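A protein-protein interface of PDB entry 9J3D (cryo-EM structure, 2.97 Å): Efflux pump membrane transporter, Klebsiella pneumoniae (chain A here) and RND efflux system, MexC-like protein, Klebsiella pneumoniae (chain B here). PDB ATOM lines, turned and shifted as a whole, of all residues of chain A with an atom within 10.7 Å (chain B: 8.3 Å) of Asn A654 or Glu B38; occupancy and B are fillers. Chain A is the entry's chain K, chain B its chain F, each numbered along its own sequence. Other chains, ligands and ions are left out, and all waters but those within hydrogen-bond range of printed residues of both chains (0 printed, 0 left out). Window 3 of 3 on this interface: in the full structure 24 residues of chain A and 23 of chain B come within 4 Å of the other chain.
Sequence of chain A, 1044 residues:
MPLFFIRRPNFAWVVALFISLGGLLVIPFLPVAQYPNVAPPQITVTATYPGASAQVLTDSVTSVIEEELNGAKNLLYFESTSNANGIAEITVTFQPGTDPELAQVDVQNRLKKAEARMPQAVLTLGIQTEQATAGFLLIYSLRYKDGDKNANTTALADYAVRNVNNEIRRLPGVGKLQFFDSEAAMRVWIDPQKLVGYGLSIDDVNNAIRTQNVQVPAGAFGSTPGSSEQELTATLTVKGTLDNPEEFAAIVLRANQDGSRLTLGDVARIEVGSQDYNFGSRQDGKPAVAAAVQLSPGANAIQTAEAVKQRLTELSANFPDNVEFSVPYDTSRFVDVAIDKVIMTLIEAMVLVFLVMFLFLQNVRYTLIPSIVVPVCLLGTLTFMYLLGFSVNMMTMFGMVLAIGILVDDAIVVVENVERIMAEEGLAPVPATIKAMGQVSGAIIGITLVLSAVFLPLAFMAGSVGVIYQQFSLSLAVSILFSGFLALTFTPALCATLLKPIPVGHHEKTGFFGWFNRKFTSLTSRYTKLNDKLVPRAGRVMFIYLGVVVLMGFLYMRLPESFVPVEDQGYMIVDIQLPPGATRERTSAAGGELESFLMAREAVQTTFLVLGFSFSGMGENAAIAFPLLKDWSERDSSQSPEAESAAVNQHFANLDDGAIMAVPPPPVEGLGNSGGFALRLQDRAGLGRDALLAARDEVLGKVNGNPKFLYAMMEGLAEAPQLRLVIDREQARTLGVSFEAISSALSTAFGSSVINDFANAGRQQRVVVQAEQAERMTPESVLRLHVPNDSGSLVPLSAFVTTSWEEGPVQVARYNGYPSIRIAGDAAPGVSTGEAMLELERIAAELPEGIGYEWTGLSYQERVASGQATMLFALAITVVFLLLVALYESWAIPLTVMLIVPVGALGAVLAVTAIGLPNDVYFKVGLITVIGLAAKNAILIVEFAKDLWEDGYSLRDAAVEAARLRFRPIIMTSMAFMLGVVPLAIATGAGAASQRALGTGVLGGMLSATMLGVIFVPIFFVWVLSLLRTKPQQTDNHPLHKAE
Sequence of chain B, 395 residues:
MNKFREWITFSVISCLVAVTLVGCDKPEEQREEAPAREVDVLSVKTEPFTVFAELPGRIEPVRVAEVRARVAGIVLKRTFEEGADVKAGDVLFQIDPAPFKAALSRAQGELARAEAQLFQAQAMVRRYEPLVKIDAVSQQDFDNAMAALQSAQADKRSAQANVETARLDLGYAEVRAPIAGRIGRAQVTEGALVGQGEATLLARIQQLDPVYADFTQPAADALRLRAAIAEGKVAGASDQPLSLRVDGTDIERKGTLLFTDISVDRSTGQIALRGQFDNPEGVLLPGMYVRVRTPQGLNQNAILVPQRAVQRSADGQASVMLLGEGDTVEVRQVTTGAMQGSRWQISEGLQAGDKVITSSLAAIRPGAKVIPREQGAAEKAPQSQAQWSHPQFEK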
ATOM      1  N   GLU A 593     -23.996  14.574  31.961  1.00  0.00           N
ATOM      2  CA  GLU A 593     -23.640  15.301  30.743  1.00  0.00           C
ATOM      3  C   GLU A 593     -24.539  16.520  30.556  1.00  0.00           C
ATOM      4  O   GLU A 593     -24.065  17.620  30.227  1.00  0.00           O
ATOM      5  CB  GLU A 593     -23.726  14.372  29.533  1.00  0.00           C
ATOM      6  CG  GLU A 593     -23.144  14.962  28.260  1.00  0.00           C
ATOM      7  CD  GLU A 593     -23.229  14.009  27.083  1.00  0.00           C
ATOM      8  OE1 GLU A 593     -23.626  12.842  27.287  1.00  0.00           O
ATOM      9  OE2 GLU A 593     -22.898  14.427  25.953  1.00  0.00           O
ATOM     10  N   ALA A 646     -33.790  25.998  21.994  1.00  0.00           N
ATOM     11  CA  ALA A 646     -33.267  25.623  20.686  1.00  0.00           C
ATOM     12  C   ALA A 646     -31.794  25.251  20.775  1.00  0.00           C
ATOM     13  O   ALA A 646     -31.355  24.277  20.157  1.00  0.00           O
ATOM     14  CB  ALA A 646     -33.476  26.762  19.689  1.00  0.00           C
ATOM     15  N   ALA A 647     -31.021  26.008  21.554  1.00  0.00           N
ATOM     16  CA  ALA A 647     -29.601  25.707  21.706  1.00  0.00           C
ATOM     17  C   ALA A 647     -29.386  24.350  22.363  1.00  0.00           C
ATOM     18  O   ALA A 647     -28.516  23.581  21.938  1.00  0.00           O
ATOM     19  CB  ALA A 647     -28.916  26.808  22.512  1.00  0.00           C
ATOM     20  N   VAL A 648     -30.163  24.041  23.403  1.00  0.00           N
ATOM     21  CA  VAL A 648     -30.014  22.759  24.087  1.00  0.00           C
ATOM     22  C   VAL A 648     -30.408  21.614  23.165  1.00  0.00           C
ATOM     23  O   VAL A 648     -29.714  20.593  23.082  1.00  0.00           O
ATOM     24  CB  VAL A 648     -30.834  22.742  25.389  1.00  0.00           C
ATOM     25  CG1 VAL A 648     -30.909  21.334  25.946  1.00  0.00           C
ATOM     26  CG2 VAL A 648     -30.214  23.678  26.409  1.00  0.00           C
ATOM     27  N   ASN A 649     -31.526  21.764  22.451  1.00  0.00           N
ATOM     28  CA  ASN A 649     -31.948  20.725  21.518  1.00  0.00           C
ATOM     29  C   ASN A 649     -30.934  20.552  20.393  1.00  0.00           C
ATOM     30  O   ASN A 649     -30.779  19.454  19.851  1.00  0.00           O
ATOM     31  CB  ASN A 649     -33.328  21.053  20.952  1.00  0.00           C
ATOM     32  CG  ASN A 649     -34.422  20.948  21.991  1.00  0.00           C
ATOM     33  OD1 ASN A 649     -34.238  20.334  23.040  1.00  0.00           O
ATOM     34  ND2 ASN A 649     -35.570  21.545  21.705  1.00  0.00           N
ATOM     35  N   GLN A 650     -30.239  21.630  20.029  1.00  0.00           N
ATOM     36  CA  GLN A 650     -29.212  21.543  18.997  1.00  0.00           C
ATOM     37  C   GLN A 650     -27.971  20.824  19.509  1.00  0.00           C
ATOM     38  O   GLN A 650     -27.377  20.014  18.790  1.00  0.00           O
ATOM     39  CB  GLN A 650     -28.857  22.946  18.508  1.00  0.00           C
ATOM     40  CG  GLN A 650     -27.902  22.989  17.333  1.00  0.00           C
ATOM     41  CD  GLN A 650     -27.579  24.409  16.909  1.00  0.00           C
ATOM     42  OE1 GLN A 650     -27.968  25.370  17.573  1.00  0.00           O
ATOM     43  NE2 GLN A 650     -26.866  24.548  15.799  1.00  0.00           N
ATOM     44  N   HIS A 651     -27.562  21.112  20.745  1.00  0.00           N
ATOM     45  CA  HIS A 651     -26.344  20.509  21.275  1.00  0.00           C
ATOM     46  C   HIS A 651     -26.507  19.009  21.480  1.00  0.00           C
ATOM     47  O   HIS A 651     -25.649  18.224  21.064  1.00  0.00           O
ATOM     48  CB  HIS A 651     -25.949  21.181  22.586  1.00  0.00           C
ATOM     49  CG  HIS A 651     -24.684  20.645  23.179  1.00  0.00           C
ATOM     50  ND1 HIS A 651     -23.444  20.885  22.627  1.00  0.00           N
ATOM     51  CD2 HIS A 651     -24.468  19.869  24.267  1.00  0.00           C
ATOM     52  CE1 HIS A 651     -22.518  20.288  23.357  1.00  0.00           C
ATOM     53  NE2 HIS A 651     -23.113  19.666  24.357  1.00  0.00           N
ATOM     54  N   PHE A 652     -27.598  18.592  22.118  1.00  0.00           N
ATOM     55  CA  PHE A 652     -27.845  17.187  22.402  1.00  0.00           C
ATOM     56  C   PHE A 652     -28.706  16.515  21.342  1.00  0.00           C
ATOM     57  O   PHE A 652     -29.332  15.490  21.625  1.00  0.00           O
ATOM     58  CB  PHE A 652     -28.497  17.031  23.777  1.00  0.00           C
ATOM     59  CG  PHE A 652     -27.575  17.331  24.923  1.00  0.00           C
ATOM     60  CD1 PHE A 652     -26.403  16.617  25.089  1.00  0.00           C
ATOM     61  CD2 PHE A 652     -27.887  18.315  25.842  1.00  0.00           C
ATOM     62  CE1 PHE A 652     -25.555  16.887  26.144  1.00  0.00           C
ATOM     63  CE2 PHE A 652     -27.043  18.588  26.898  1.00  0.00           C
ATOM     64  CZ  PHE A 652     -25.876  17.871  27.050  1.00  0.00           C
ATOM     65  N   ALA A 653     -28.754  17.069  20.129  1.00  0.00           N
ATOM     66  CA  ALA A 653     -29.513  16.431  19.059  1.00  0.00           C
ATOM     67  C   ALA A 653     -28.911  15.089  18.670  1.00  0.00           C
ATOM     68  O   ALA A 653     -29.599  14.245  18.086  1.00  0.00           O
ATOM     69  CB  ALA A 653     -29.581  17.347  17.838  1.00  0.00           C
ATOM     70  N   ASN A 654     -27.637  14.874  18.981  1.00  0.00           N
ATOM     71  CA  ASN A 654     -26.929  13.652  18.630  1.00  0.00           C
ATOM     72  C   ASN A 654     -26.476  12.918  19.888  1.00  0.00           C
ATOM     73  O   ASN A 654     -25.342  12.445  19.986  1.00  0.00           O
ATOM     74  CB  ASN A 654     -25.750  13.960  17.709  1.00  0.00           C
ATOM     75  CG  ASN A 654     -25.081  12.709  17.169  1.00  0.00           C
ATOM     76  OD1 ASN A 654     -25.418  12.227  16.088  1.00  0.00           O
ATOM     77  ND2 ASN A 654     -24.122  12.182  17.919  1.00  0.00           N
ATOM     78  N   LEU A 655     -27.356  12.835  20.883  1.00  0.00           N
ATOM     79  CA  LEU A 655     -27.057  12.038  22.064  1.00  0.00           C
ATOM     80  C   LEU A 655     -27.179  10.561  21.728  1.00  0.00           C
ATOM     81  O   LEU A 655     -28.172  10.125  21.138  1.00  0.00           O
ATOM     82  CB  LEU A 655     -27.989  12.400  23.216  1.00  0.00           C
ATOM     83  CG  LEU A 655     -27.484  11.986  24.601  1.00  0.00           C
ATOM     84  CD1 LEU A 655     -25.965  12.025  24.669  1.00  0.00           C
ATOM     85  CD2 LEU A 655     -28.086  12.861  25.678  1.00  0.00           C
ATOM     86  N   ASP A 656     -26.164   9.787  22.110  1.00  0.00           N
ATOM     87  CA  ASP A 656     -26.082   8.405  21.657  1.00  0.00           C
ATOM     88  C   ASP A 656     -26.807   7.448  22.594  1.00  0.00           C
ATOM     89  O   ASP A 656     -27.230   6.369  22.165  1.00  0.00           O
ATOM     90  CB  ASP A 656     -24.616   8.006  21.501  1.00  0.00           C
ATOM     91  CG  ASP A 656     -23.862   8.006  22.815  1.00  0.00           C
ATOM     92  OD1 ASP A 656     -22.698   7.553  22.825  1.00  0.00           O
ATOM     93  OD2 ASP A 656     -24.415   8.473  23.832  1.00  0.00           O
ATOM     94  N   ASP A 657     -26.960   7.813  23.862  1.00  0.00           N
ATOM     95  CA  ASP A 657     -27.585   6.957  24.868  1.00  0.00           C
ATOM     96  C   ASP A 657     -28.810   7.678  25.419  1.00  0.00           C
ATOM     97  O   ASP A 657     -28.720   8.435  26.387  1.00  0.00           O
ATOM     98  CB  ASP A 657     -26.584   6.610  25.973  1.00  0.00           C
ATOM     99  CG  ASP A 657     -27.097   5.535  26.910  1.00  0.00           C
ATOM    100  OD1 ASP A 657     -28.054   4.826  26.535  1.00  0.00           O
ATOM    101  OD2 ASP A 657     -26.542   5.399  28.022  1.00  0.00           O
ATOM    102  N   GLY A 658     -29.958   7.437  24.801  1.00  0.00           N
ATOM    103  CA  GLY A 658     -31.196   8.034  25.259  1.00  0.00           C
ATOM    104  C   GLY A 658     -31.601   9.249  24.448  1.00  0.00           C
ATOM    105  O   GLY A 658     -31.151   9.474  23.320  1.00  0.00           O
ATOM    106  N   ALA A 659     -32.477  10.050  25.049  1.00  0.00           N
ATOM    107  CA  ALA A 659     -33.043  11.222  24.399  1.00  0.00           C
ATOM    108  C   ALA A 659     -33.171  12.369  25.389  1.00  0.00           C
ATOM    109  O   ALA A 659     -33.578  12.171  26.539  1.00  0.00           O
ATOM    110  CB  ALA A 659     -34.412  10.906  23.792  1.00  0.00           C
ATOM    111  N   ILE A 660     -32.828  13.568  24.926  1.00  0.00           N
ATOM    112  CA  ILE A 660     -32.972  14.807  25.683  1.00  0.00           C
ATOM    113  C   ILE A 660     -33.916  15.701  24.898  1.00  0.00           C
ATOM    114  O   ILE A 660     -33.778  15.827  23.675  1.00  0.00           O
ATOM    115  CB  ILE A 660     -31.620  15.507  25.896  1.00  0.00           C
ATOM    116  CG1 ILE A 660     -30.783  14.778  26.942  1.00  0.00           C
ATOM    117  CG2 ILE A 660     -31.827  16.951  26.313  1.00  0.00           C
ATOM    118  CD1 ILE A 660     -31.576  14.199  28.056  1.00  0.00           C
ATOM    119  N   MET A 661     -34.877  16.316  25.584  1.00  0.00           N
ATOM    120  CA  MET A 661     -35.803  17.229  24.921  1.00  0.00           C
ATOM    121  C   MET A 661     -36.104  18.417  25.820  1.00  0.00           C
ATOM    122  O   MET A 661     -36.562  18.239  26.950  1.00  0.00           O
ATOM    123  CB  MET A 661     -37.096  16.510  24.531  1.00  0.00           C
ATOM    124  CG  MET A 661     -38.124  17.411  23.872  1.00  0.00           C
ATOM    125  SD  MET A 661     -39.714  16.603  23.607  1.00  0.00           S
ATOM    126  CE  MET A 661     -39.248  14.877  23.711  1.00  0.00           C
ATOM    127  N   ALA B  36     -26.981  11.990   8.867  1.00  0.00           N
ATOM    128  CA  ALA B  36     -26.426  10.757   9.413  1.00  0.00           C
ATOM    129  C   ALA B  36     -25.893  10.981  10.823  1.00  0.00           C
ATOM    130  O   ALA B  36     -25.040  11.838  11.044  1.00  0.00           O
ATOM    131  CB  ALA B  36     -25.331  10.222   8.508  1.00  0.00           C
ATOM    132  N   ARG B  37     -26.401  10.202  11.772  1.00  0.00           N
ATOM    133  CA  ARG B  37     -26.015  10.356  13.167  1.00  0.00           C
ATOM    134  C   ARG B  37     -24.739   9.579  13.461  1.00  0.00           C
ATOM    135  O   ARG B  37     -24.592   8.424  13.057  1.00  0.00           O
ATOM    136  CB  ARG B  37     -27.140   9.876  14.082  1.00  0.00           C
ATOM    137  CG  ARG B  37     -28.287  10.862  14.213  1.00  0.00           C
ATOM    138  CD  ARG B  37     -29.300  10.405  15.249  1.00  0.00           C
ATOM    139  NE  ARG B  37     -28.667  10.040  16.510  1.00  0.00           N
ATOM    140  CZ  ARG B  37     -28.929  10.617  17.675  1.00  0.00           C
ATOM    141  NH1 ARG B  37     -29.807  11.602  17.776  1.00  0.00           N
ATOM    142  NH2 ARG B  37     -28.296  10.197  18.765  1.00  0.00           N
ATOM    143  N   GLU B  38     -23.815  10.224  14.168  1.00  0.00           N
ATOM    144  CA  GLU B  38     -22.572   9.565  14.545  1.00  0.00           C
ATOM    145  C   GLU B  38     -22.837   8.531  15.630  1.00  0.00           C
ATOM    146  O   GLU B  38     -23.497   8.822  16.631  1.00  0.00           O
ATOM    147  CB  GLU B  38     -21.550  10.590  15.028  1.00  0.00           C
ATOM    148  CG  GLU B  38     -21.034  11.510  13.938  1.00  0.00           C
ATOM    149  CD  GLU B  38     -19.882  12.376  14.406  1.00  0.00           C
ATOM    150  OE1 GLU B  38     -19.418  12.183  15.549  1.00  0.00           O
ATOM    151  OE2 GLU B  38     -19.440  13.250  13.631  1.00  0.00           O
ATOM    152  N   VAL B  39     -22.318   7.322  15.432  1.00  0.00           N
ATOM    153  CA  VAL B  39     -22.563   6.203  16.333  1.00  0.00           C
ATOM    154  C   VAL B  39     -21.235   5.573  16.719  1.00  0.00           C
ATOM    155  O   VAL B  39     -20.288   5.558  15.925  1.00  0.00           O
ATOM    156  CB  VAL B  39     -23.495   5.153  15.693  1.00  0.00           C
ATOM    157  CG1 VAL B  39     -24.838   5.773  15.368  1.00  0.00           C
ATOM    158  CG2 VAL B  39     -22.864   4.572  14.442  1.00  0.00           C
ATOM    159  N   ASP B  40     -21.161   5.065  17.945  1.00  0.00           N
ATOM    160  CA  ASP B  40     -19.990   4.322  18.388  1.00  0.00           C
ATOM    161  C   ASP B  40     -20.085   2.888  17.889  1.00  0.00           C
ATOM    162  O   ASP B  40     -21.128   2.241  18.024  1.00  0.00           O
ATOM    163  CB  ASP B  40     -19.877   4.353  19.912  1.00  0.00           C
ATOM    164  CG  ASP B  40     -19.463   5.712  20.437  1.00  0.00           C
ATOM    165  OD1 ASP B  40     -18.828   6.474  19.681  1.00  0.00           O
ATOM    166  OD2 ASP B  40     -19.769   6.018  21.607  1.00  0.00           O
ATOM    167  N   VAL B  41     -18.994   2.392  17.313  1.00  0.00           N
ATOM    168  CA  VAL B  41     -18.959   1.076  16.687  1.00  0.00           C
ATOM    169  C   VAL B  41     -17.926   0.225  17.408  1.00  0.00           C
ATOM    170  O   VAL B  41     -16.803   0.680  17.652  1.00  0.00           O
ATOM    171  CB  VAL B  41     -18.633   1.171  15.187  1.00  0.00           C
ATOM    172  CG1 VAL B  41     -18.843  -0.171  14.520  1.00  0.00           C
ATOM    173  CG2 VAL B  41     -19.483   2.237  14.530  1.00  0.00           C
ATOM    174  N   ILE B 357     -23.172  -1.769  16.306  1.00  0.00           N
ATOM    175  CA  ILE B 357     -23.460  -0.409  16.745  1.00  0.00           C
ATOM    176  C   ILE B 357     -23.893  -0.450  18.202  1.00  0.00           C
ATOM    177  O   ILE B 357     -24.806  -1.198  18.570  1.00  0.00           O
ATOM    178  CB  ILE B 357     -24.544   0.231  15.863  1.00  0.00           C
ATOM    179  CG1 ILE B 357     -24.139   0.212  14.388  1.00  0.00           C
ATOM    180  CG2 ILE B 357     -24.820   1.653  16.312  1.00  0.00           C
ATOM    181  CD1 ILE B 357     -22.677   0.517  14.134  1.00  0.00           C
ATOM    182  N   SER B 359     -24.737   2.473  20.052  1.00  0.00           N
ATOM    183  CA  SER B 359     -25.245   3.784  20.420  1.00  0.00           C
ATOM    184  C   SER B 359     -26.326   4.229  19.443  1.00  0.00           C
ATOM    185  O   SER B 359     -26.423   3.732  18.318  1.00  0.00           O
ATOM    186  CB  SER B 359     -24.108   4.807  20.465  1.00  0.00           C
ATOM    187  OG  SER B 359     -23.637   5.099  19.162  1.00  0.00           O
ATOM    188  N   SER B 360     -27.146   5.178  19.896  1.00  0.00           N
ATOM    189  CA  SER B 360     -28.216   5.785  19.104  1.00  0.00           C
ATOM    190  C   SER B 360     -29.179   4.753  18.535  1.00  0.00           C
ATOM    191  O   SER B 360     -29.835   5.008  17.522  1.00  0.00           O
ATOM    192  CB  SER B 360     -27.647   6.648  17.973  1.00  0.00           C
ATOM    193  OG  SER B 360     -26.901   7.738  18.485  1.00  0.00           O
ATOM    194  N   LEU B 361     -29.291   3.594  19.187  1.00  0.00           N
ATOM    195  CA  LEU B 361     -30.014   2.474  18.596  1.00  0.00           C
ATOM    196  C   LEU B 361     -31.491   2.793  18.403  1.00  0.00           C
ATOM    197  O   LEU B 361     -32.088   2.414  17.389  1.00  0.00           O
ATOM    198  CB  LEU B 361     -29.838   1.231  19.461  1.00  0.00           C
ATOM    199  CG  LEU B 361     -28.411   0.689  19.506  1.00  0.00           C
ATOM    200  CD1 LEU B 361     -28.362  -0.591  20.310  1.00  0.00           C
ATOM    201  CD2 LEU B 361     -27.881   0.460  18.103  1.00  0.00           C
ATOM    202  N   ALA B 363     -32.733   5.559  17.681  1.00  0.00           N
ATOM    203  CA  ALA B 363     -32.880   6.582  16.658  1.00  0.00           C
ATOM    204  C   ALA B 363     -32.452   6.121  15.271  1.00  0.00           C
ATOM    205  O   ALA B 363     -32.392   6.950  14.357  1.00  0.00           O
ATOM    206  CB  ALA B 363     -32.082   7.832  17.042  1.00  0.00           C
ATOM    207  N   ILE B 364     -32.156   4.838  15.087  1.00  0.00           N
ATOM    208  CA  ILE B 364     -31.694   4.310  13.810  1.00  0.00           C
ATOM    209  C   ILE B 364     -32.666   3.245  13.327  1.00  0.00           C
ATOM    210  O   ILE B 364     -33.063   2.359  14.092  1.00  0.00           O
ATOM    211  CB  ILE B 364     -30.270   3.733  13.912  1.00  0.00           C
ATOM    212  CG1 ILE B 364     -29.293   4.797  14.401  1.00  0.00           C
ATOM    213  CG2 ILE B 364     -29.820   3.188  12.573  1.00  0.00           C
ATOM    214  CD1 ILE B 364     -28.042   4.219  15.015  1.00  0.00           C
ATOM    215  N   LYS B 369     -28.339   5.262   6.617  1.00  0.00           N
ATOM    216  CA  LYS B 369     -26.924   5.601   6.569  1.00  0.00           C
ATOM    217  C   LYS B 369     -26.504   6.314   7.847  1.00  0.00           C
ATOM    218  O   LYS B 369     -27.190   7.221   8.324  1.00  0.00           O
ATOM    219  CB  LYS B 369     -26.626   6.480   5.354  1.00  0.00           C
ATOM    220  CG  LYS B 369     -25.805   5.794   4.271  1.00  0.00           C
ATOM    221  CD  LYS B 369     -26.397   4.451   3.873  1.00  0.00           C
ATOM    222  CE  LYS B 369     -27.781   4.601   3.257  1.00  0.00           C
ATOM    223  NZ  LYS B 369     -28.477   3.290   3.136  1.00  0.00           N
ATOM    224  N   VAL B 370     -25.367   5.894   8.401  1.00  0.00           N
ATOM    225  CA  VAL B 370     -24.832   6.460   9.630  1.00  0.00           C
ATOM    226  C   VAL B 370     -23.344   6.717   9.447  1.00  0.00           C
ATOM    227  O   VAL B 370     -22.699   6.167   8.552  1.00  0.00           O
ATOM    228  CB  VAL B 370     -25.068   5.544  10.848  1.00  0.00           C
ATOM    229  CG1 VAL B 370     -26.551   5.444  11.158  1.00  0.00           C
ATOM    230  CG2 VAL B 370     -24.478   4.172  10.594  1.00  0.00           C
ATOM    231  N   ILE B 371     -22.802   7.567  10.313  1.00  0.00           N
ATOM    232  CA  ILE B 371     -21.383   7.907  10.306  1.00  0.00           C
ATOM    233  C   ILE B 371     -20.722   7.172  11.469  1.00  0.00           C
ATOM    234  O   ILE B 371     -20.993   7.507  12.633  1.00  0.00           O
ATOM    235  CB  ILE B 371     -21.163   9.421  10.412  1.00  0.00           C
ATOM    236  CG1 ILE B 371     -21.763  10.131   9.199  1.00  0.00           C
ATOM    237  CG2 ILE B 371     -19.683   9.734  10.535  1.00  0.00           C
ATOM    238  CD1 ILE B 371     -21.761  11.637   9.310  1.00  0.00           C
ATOM    239  N   PRO B 372     -19.869   6.182  11.214  1.00  0.00           N
ATOM    240  CA  PRO B 372     -19.253   5.437  12.319  1.00  0.00           C
ATOM    241  C   PRO B 372     -18.206   6.277  13.035  1.00  0.00           C
ATOM    242  O   PRO B 372     -17.420   6.986  12.404  1.00  0.00           O
ATOM    243  CB  PRO B 372     -18.625   4.229  11.619  1.00  0.00           C
ATOM    244  CG  PRO B 372     -18.314   4.727  10.251  1.00  0.00           C
ATOM    245  CD  PRO B 372     -19.411   5.702   9.900  1.00  0.00           C
ATOM    246  N   ARG B 373     -18.106   6.214  14.353  1.00  0.00           N
ATOM    247  CA  ARG B 373     -17.141   7.131  15.020  1.00  0.00           C
ATOM    248  C   ARG B 373     -15.825   6.409  15.292  1.00  0.00           C
ATOM    249  O   ARG B 373     -14.801   7.105  15.345  1.00  0.00           O
ATOM    250  CB  ARG B 373     -17.674   7.667  16.347  1.00  0.00           C
ATOM    251  CG  ARG B 373     -18.540   8.910  16.220  1.00  0.00           C
ATOM    252  CD  ARG B 373     -18.985   9.406  17.581  1.00  0.00           C
ATOM    253  NE  ARG B 373     -20.039   8.584  18.154  1.00  0.00           N
ATOM    254  CZ  ARG B 373     -21.180   9.057  18.634  1.00  0.00           C
ATOM    255  NH1 ARG B 373     -21.424  10.354  18.601  1.00  0.00           N
ATOM    256  NH2 ARG B 373     -22.081   8.231  19.135  1.00  0.00           N
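NH1 of Arg B37 sits at hydrogen-bond distance from O of Ala A653 (2.7 Å).
The backbone NH (N) of Glu B38 lies within hydrogen-bond range of the side-chain amide oxygen (OD1) of Asn A654, at 3.2 Å.
O of Asp A656 sits at hydrogen-bond distance from N of Ser B360 (2.6 Å).
The side-chain amide nitrogen (ND2) of Asn A654 lies close to the guanidinium group (NH1) of Arg B373 (3.3 Å).
NH2 of Arg B373 is in salt-bridge range of OD1 of Asp A656 (3.8 Å).
O of Leu A655 sits close to NH2 of Arg B37, 2.4 Å away.
The guanidinium group (NH2) of Arg B37 sits at hydrogen-bond distance from the side-chain hydroxyl (OG) of Ser B360, 2.8 Å away.
The backbone NH (N) of Ile B371 lies within hydrogen-bond range of the backbone carbonyl oxygen (O) of Arg B37 (3.4 Å).
O of Glu B38 sits at hydrogen-bond distance from NH2 of Arg B373, at 2.9 Å.
O of Val B39 lies within hydrogen-bond range of N of Arg B373 (2.8 Å).
N of Asp B40 sits at hydrogen-bond distance from OG of Ser B359, at 2.8 Å.
OG of Ser B359 sits at hydrogen-bond distance from NH2 of Arg B373 (3.5 Å).
Among the printed residues, merely in contact across the chains: Asn A654 with Arg B37 (3.5 Å), Leu A655 with Ser B360 (3.8 Å), Asp A656 with Arg B37 (3.99 Å), Asp A656 with Asp B40 (3.5 Å) and Asp A656 with Ser B359 (3.4 Å).
Ala A647 touches none of the printed residues of chain B.
Of chain B, only Arg B37 (2.7 Å) comes within 4 Å of Ala A653.
Of chain B, only Arg B37 (3.5 Å), Glu B38 (3.2 Å) and Arg B373 (3.3 Å) come within 4 Å of Asn A654.
Of the printed residues of chain A, Arg B37 touches Ala A653 (2.7 Å), Asn A654 (3.5 Å), Leu A655 (2.4 Å) and Asp A656 (3.99 Å).
Of chain A, only Asn A654 comes within 4 Å of Glu B38.
Printed residues of chain A within 4 Å of Asp B40: Asp A656.
Ile B357 touches none of the printed residues of chain A.
Of the printed residues of chain A, Ser B359 touches Asp A656.
Of the printed residues of chain A, Ser B360 touches Leu A655 (3.8 Å) and Asp A656 (2.6 Å).
Printed residues of chain A within 4 Å of Arg B373: Asn A654 (3.3 Å) and Asp A656 (3.5 Å).
The nearest residue of chain B that does not touch Asn A654 is Ala B36 (5.1 Å).
The nearest residue of chain A that does not touch Glu B38 is Asp A656 (5.1 Å).
The nearest printed residue of chain B that does not touch Leu A655 is Ala B363 (6.1 Å).
Along chain A the printed residues that touch a printed residue of chain B span positions 653 to 656.
Along chain B the printed residues that touch a printed residue of chain A span positions 37 to 373.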
